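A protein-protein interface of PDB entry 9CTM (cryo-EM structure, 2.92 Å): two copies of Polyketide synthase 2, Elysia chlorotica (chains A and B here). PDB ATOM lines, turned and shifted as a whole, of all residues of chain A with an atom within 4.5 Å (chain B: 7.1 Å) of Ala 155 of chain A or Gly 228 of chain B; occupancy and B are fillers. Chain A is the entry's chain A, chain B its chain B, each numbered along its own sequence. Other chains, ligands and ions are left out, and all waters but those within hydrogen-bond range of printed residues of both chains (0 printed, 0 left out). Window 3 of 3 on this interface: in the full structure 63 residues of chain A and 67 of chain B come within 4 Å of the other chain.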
ATOM      1  N   ASP A 153     -28.939  -6.152  37.832  1.00  0.00           N
ATOM      2  CA  ASP A 153     -28.558  -4.742  37.885  1.00  0.00           C
ATOM      3  C   ASP A 153     -27.279  -4.479  37.094  1.00  0.00           C
ATOM      4  O   ASP A 153     -26.857  -3.319  37.007  1.00  0.00           O
ATOM      5  CB  ASP A 153     -28.368  -4.220  39.321  1.00  0.00           C
ATOM      6  CG  ASP A 153     -29.676  -4.117  40.081  1.00  0.00           C
ATOM      7  OD1 ASP A 153     -30.746  -4.179  39.440  1.00  0.00           O
ATOM      8  OD2 ASP A 153     -29.634  -3.974  41.322  1.00  0.00           O
ATOM      9  N   ASP A 154     -26.649  -5.503  36.519  1.00  0.00           N
ATOM     10  CA  ASP A 154     -25.473  -5.336  35.676  1.00  0.00           C
ATOM     11  C   ASP A 154     -25.825  -5.223  34.198  1.00  0.00           C
ATOM     12  O   ASP A 154     -24.921  -5.192  33.358  1.00  0.00           O
ATOM     13  CB  ASP A 154     -24.503  -6.504  35.882  1.00  0.00           C
ATOM     14  CG  ASP A 154     -23.585  -6.301  37.074  1.00  0.00           C
ATOM     15  OD1 ASP A 154     -23.698  -5.256  37.748  1.00  0.00           O
ATOM     16  OD2 ASP A 154     -22.748  -7.190  37.336  1.00  0.00           O
ATOM     17  N   ALA A 155     -27.117  -5.163  33.864  1.00  0.00           N
ATOM     18  CA  ALA A 155     -27.516  -5.077  32.463  1.00  0.00           C
ATOM     19  C   ALA A 155     -26.939  -3.831  31.802  1.00  0.00           C
ATOM     20  O   ALA A 155     -26.482  -3.883  30.652  1.00  0.00           O
ATOM     21  CB  ALA A 155     -29.040  -5.081  32.358  1.00  0.00           C
ATOM     22  N   TYR A 156     -26.911  -2.713  32.528  1.00  0.00           N
ATOM     23  CA  TYR A 156     -26.444  -1.439  31.993  1.00  0.00           C
ATOM     24  C   TYR A 156     -25.069  -1.557  31.343  1.00  0.00           C
ATOM     25  O   TYR A 156     -24.638  -0.648  30.626  1.00  0.00           O
ATOM     26  CB  TYR A 156     -26.415  -0.386  33.104  1.00  0.00           C
ATOM     27  CG  TYR A 156     -27.789   0.016  33.589  1.00  0.00           C
ATOM     28  CD1 TYR A 156     -28.667   0.692  32.753  1.00  0.00           C
ATOM     29  CD2 TYR A 156     -28.214  -0.289  34.876  1.00  0.00           C
ATOM     30  CE1 TYR A 156     -29.925   1.062  33.184  1.00  0.00           C
ATOM     31  CE2 TYR A 156     -29.473   0.077  35.316  1.00  0.00           C
ATOM     32  CZ  TYR A 156     -30.323   0.751  34.467  1.00  0.00           C
ATOM     33  OH  TYR A 156     -31.577   1.116  34.900  1.00  0.00           O
ATOM     34  N   MET A 157     -24.377  -2.674  31.579  1.00  0.00           N
ATOM     35  CA  MET A 157     -23.086  -2.902  30.945  1.00  0.00           C
ATOM     36  C   MET A 157     -23.164  -2.740  29.435  1.00  0.00           C
ATOM     37  O   MET A 157     -22.195  -2.291  28.813  1.00  0.00           O
ATOM     38  CB  MET A 157     -22.569  -4.299  31.294  1.00  0.00           C
ATOM     39  CG  MET A 157     -21.430  -4.294  32.307  1.00  0.00           C
ATOM     40  SD  MET A 157     -20.633  -5.895  32.568  1.00  0.00           S
ATOM     41  CE  MET A 157     -20.379  -6.465  30.891  1.00  0.00           C
ATOM     42  N   VAL A 158     -24.309  -3.076  28.827  1.00  0.00           N
ATOM     43  CA  VAL A 158     -24.424  -2.934  27.375  1.00  0.00           C
ATOM     44  C   VAL A 158     -24.097  -1.506  26.963  1.00  0.00           C
ATOM     45  O   VAL A 158     -23.399  -1.274  25.968  1.00  0.00           O
ATOM     46  CB  VAL A 158     -25.825  -3.346  26.875  1.00  0.00           C
ATOM     47  CG1 VAL A 158     -25.971  -4.853  26.837  1.00  0.00           C
ATOM     48  CG2 VAL A 158     -26.923  -2.715  27.718  1.00  0.00           C
ATOM     49  N   THR B 222     -24.612 -13.667  27.919  1.00  0.00           N
ATOM     50  CA  THR B 222     -24.787 -12.477  27.094  1.00  0.00           C
ATOM     51  C   THR B 222     -26.250 -12.292  26.711  1.00  0.00           C
ATOM     52  O   THR B 222     -26.767 -11.168  26.711  1.00  0.00           O
ATOM     53  CB  THR B 222     -23.912 -12.566  25.842  1.00  0.00           C
ATOM     54  OG1 THR B 222     -22.531 -12.460  26.211  1.00  0.00           O
ATOM     55  CG2 THR B 222     -24.258 -11.451  24.863  1.00  0.00           C
ATOM     56  N   THR B 223     -26.936 -13.388  26.377  1.00  0.00           N
ATOM     57  CA  THR B 223     -28.363 -13.304  26.085  1.00  0.00           C
ATOM     58  C   THR B 223     -29.145 -12.857  27.314  1.00  0.00           C
ATOM     59  O   THR B 223     -30.071 -12.045  27.210  1.00  0.00           O
ATOM     60  CB  THR B 223     -28.876 -14.653  25.581  1.00  0.00           C
ATOM     61  OG1 THR B 223     -28.380 -14.894  24.259  1.00  0.00           O
ATOM     62  CG2 THR B 223     -30.397 -14.675  25.556  1.00  0.00           C
ATOM     63  N   LYS B 224     -28.787 -13.379  28.490  1.00  0.00           N
ATOM     64  CA  LYS B 224     -29.434 -12.930  29.721  1.00  0.00           C
ATOM     65  C   LYS B 224     -29.198 -11.441  29.953  1.00  0.00           C
ATOM     66  O   LYS B 224     -30.112 -10.711  30.356  1.00  0.00           O
ATOM     67  CB  LYS B 224     -28.919 -13.741  30.910  1.00  0.00           C
ATOM     68  CG  LYS B 224     -29.777 -14.942  31.275  1.00  0.00           C
ATOM     69  CD  LYS B 224     -29.756 -15.188  32.778  1.00  0.00           C
ATOM     70  CE  LYS B 224     -30.729 -14.279  33.519  1.00  0.00           C
ATOM     71  NZ  LYS B 224     -32.135 -14.427  33.048  1.00  0.00           N
ATOM     72  N   LEU B 225     -27.970 -10.978  29.712  1.00  0.00           N
ATOM     73  CA  LEU B 225     -27.655  -9.559  29.855  1.00  0.00           C
ATOM     74  C   LEU B 225     -28.489  -8.705  28.910  1.00  0.00           C
ATOM     75  O   LEU B 225     -29.032  -7.669  29.311  1.00  0.00           O
ATOM     76  CB  LEU B 225     -26.160  -9.347  29.617  1.00  0.00           C
ATOM     77  CG  LEU B 225     -25.638  -7.908  29.646  1.00  0.00           C
ATOM     78  CD1 LEU B 225     -24.551  -7.693  30.681  1.00  0.00           C
ATOM     79  CD2 LEU B 225     -25.067  -7.618  28.269  1.00  0.00           C
ATOM     80  N   PHE B 226     -28.617  -9.131  27.655  1.00  0.00           N
ATOM     81  CA  PHE B 226     -29.446  -8.388  26.714  1.00  0.00           C
ATOM     82  C   PHE B 226     -30.899  -8.368  27.171  1.00  0.00           C
ATOM     83  O   PHE B 226     -31.566  -7.328  27.103  1.00  0.00           O
ATOM     84  CB  PHE B 226     -29.334  -9.004  25.319  1.00  0.00           C
ATOM     85  CG  PHE B 226     -28.072  -8.636  24.573  1.00  0.00           C
ATOM     86  CD1 PHE B 226     -27.197  -7.668  25.051  1.00  0.00           C
ATOM     87  CD2 PHE B 226     -27.769  -9.263  23.376  1.00  0.00           C
ATOM     88  CE1 PHE B 226     -26.049  -7.344  24.352  1.00  0.00           C
ATOM     89  CE2 PHE B 226     -26.624  -8.941  22.674  1.00  0.00           C
ATOM     90  CZ  PHE B 226     -25.764  -7.980  23.162  1.00  0.00           C
ATOM     91  N   MET B 227     -31.407  -9.508  27.644  1.00  0.00           N
ATOM     92  CA  MET B 227     -32.778  -9.555  28.140  1.00  0.00           C
ATOM     93  C   MET B 227     -32.970  -8.632  29.335  1.00  0.00           C
ATOM     94  O   MET B 227     -34.063  -8.088  29.531  1.00  0.00           O
ATOM     95  CB  MET B 227     -33.148 -10.990  28.520  1.00  0.00           C
ATOM     96  CG  MET B 227     -34.639 -11.284  28.437  1.00  0.00           C
ATOM     97  SD  MET B 227     -35.128 -12.941  28.977  1.00  0.00           S
ATOM     98  CE  MET B 227     -33.551 -13.747  29.260  1.00  0.00           C
ATOM     99  N   GLY B 228     -31.924  -8.449  30.143  1.00  0.00           N
ATOM    100  CA  GLY B 228     -32.037  -7.573  31.297  1.00  0.00           C
ATOM    101  C   GLY B 228     -32.446  -6.158  30.935  1.00  0.00           C
ATOM    102  O   GLY B 228     -33.052  -5.456  31.750  1.00  0.00           O
ATOM    103  N   MET B 229     -32.128  -5.720  29.718  1.00  0.00           N
ATOM    104  CA  MET B 229     -32.490  -4.392  29.238  1.00  0.00           C
ATOM    105  C   MET B 229     -33.733  -4.407  28.356  1.00  0.00           C
ATOM    106  O   MET B 229     -34.015  -3.409  27.685  1.00  0.00           O
ATOM    107  CB  MET B 229     -31.317  -3.772  28.475  1.00  0.00           C
ATOM    108  CG  MET B 229     -30.229  -3.217  29.378  1.00  0.00           C
ATOM    109  SD  MET B 229     -30.472  -1.474  29.770  1.00  0.00           S
ATOM    110  CE  MET B 229     -29.026  -0.748  29.006  1.00  0.00           C
ATOM    111  N   ASN B 230     -34.478  -5.513  28.339  1.00  0.00           N
ATOM    112  CA  ASN B 230     -35.718  -5.641  27.581  1.00  0.00           C
ATOM    113  C   ASN B 230     -35.491  -5.619  26.074  1.00  0.00           C
ATOM    114  O   ASN B 230     -36.421  -5.335  25.312  1.00  0.00           O
ATOM    115  CB  ASN B 230     -36.718  -4.545  27.969  1.00  0.00           C
ATOM    116  CG  ASN B 230     -36.957  -4.477  29.465  1.00  0.00           C
ATOM    117  OD1 ASN B 230     -36.947  -5.496  30.154  1.00  0.00           O
ATOM    118  ND2 ASN B 230     -37.171  -3.270  29.975  1.00  0.00           N
ATOM    119  N   PHE B 231     -34.270  -5.909  25.620  1.00  0.00           N
ATOM    120  CA  PHE B 231     -34.002  -5.932  24.185  1.00  0.00           C
ATOM    121  C   PHE B 231     -34.787  -7.042  23.496  1.00  0.00           C
ATOM    122  O   PHE B 231     -35.397  -6.824  22.443  1.00  0.00           O
ATOM    123  CB  PHE B 231     -32.502  -6.113  23.933  1.00  0.00           C
ATOM    124  CG  PHE B 231     -31.661  -4.921  24.310  1.00  0.00           C
ATOM    125  CD1 PHE B 231     -32.174  -3.634  24.265  1.00  0.00           C
ATOM    126  CD2 PHE B 231     -30.344  -5.095  24.705  1.00  0.00           C
ATOM    127  CE1 PHE B 231     -31.391  -2.548  24.608  1.00  0.00           C
ATOM    128  CE2 PHE B 231     -29.558  -4.013  25.049  1.00  0.00           C
ATOM    129  CZ  PHE B 231     -30.082  -2.738  25.001  1.00  0.00           C
ATOM    130  N   LEU B 232     -34.785  -8.238  24.076  1.00  0.00           N
ATOM    131  CA  LEU B 232     -35.383  -9.404  23.446  1.00  0.00           C
ATOM    132  C   LEU B 232     -36.857  -9.526  23.811  1.00  0.00           C
ATOM    133  O   LEU B 232     -37.278  -9.167  24.914  1.00  0.00           O
ATOM    134  CB  LEU B 232     -34.645 -10.678  23.860  1.00  0.00           C
ATOM    135  CG  LEU B 232     -33.117 -10.600  23.855  1.00  0.00           C
ATOM    136  CD1 LEU B 232     -32.517 -11.906  24.350  1.00  0.00           C
ATOM    137  CD2 LEU B 232     -32.597 -10.263  22.466  1.00  0.00           C
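O of Asp 154 of chain A touches CD1 of Leu 225 of chain B, 3.7 Å away. Ala 155 of chain A touches Leu 225 of chain B. Gly 228 of chain B touches Ala 155 of chain A (C to CB, 3.8 Å). Met 229 of chain B touches Ala 155 of chain A. Met 157 of chain A touches Leu 225 of chain B. CG1 of Val 158 of chain A touches CD2 of Leu 225 of chain B (3.2 Å). Val 158 of chain A touches Phe 226 of chain B. Val 158 of chain A touches Met 229 of chain B (CG2 to CE, 3.2 Å). Val 158 of chain A touches Phe 231 of chain B.
Of the 6 printed residues of chain A, 4 touch a printed residue of chain B. Printed residues of chain A that touch a printed residue of chain B: Asp 154, Ala 155, Met 157 and Val 158. Hydrophobic or aromatic side chains of chain A within 4 Å of the printed part of chain B: Ala 155, Met 157 and Val 158. Printed residues of chain B that touch a printed residue of chain A: Leu 225, Phe 226, Gly 228, Met 229 and Phe 231. Hydrophobic or aromatic side chains of chain B that line the printed part of chain A: Leu 225, Phe 226, Met 229 and Phe 231.
N of Phe 231 of chain B is in hydrogen-bond range of O of Phe 226 of chain B, 3.4 Å away.
No position is printed for both chains.
Of the printed residues of chain B, Asp 154 of chain A touches Leu 225. Of the printed residues of chain B, Ala 155 of chain A touches Leu 225 (3.998 Å), Gly 228 (3.8 Å) and Met 229 (3.7 Å). Of the printed residues of chain B, Met 157 of chain A touches Leu 225 (3.98 Å). Of the printed residues of chain B, Val 158 of chain A touches Leu 225, Phe 226, Met 229 and Phe 231. Printed residues of chain A within 4 Å of Phe 226 of chain B: Val 158 (3.5 Å). Gly 228 of chain B touches one residue of chain A. Of the printed residues of chain A, Met 229 of chain B touches Ala 155 and Val 158. The nearest printed residue of chain B that does not touch Ala 155 of chain A is Lys 224 of chain B (6.1 Å). The nearest printed residue of chain A that does not touch Gly 228 of chain B is Tyr 156 of chain A (6.7 Å). The nearest printed residue of chain A that does not touch Phe 231 of chain B is Ala 155 of chain A (6.4 Å).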
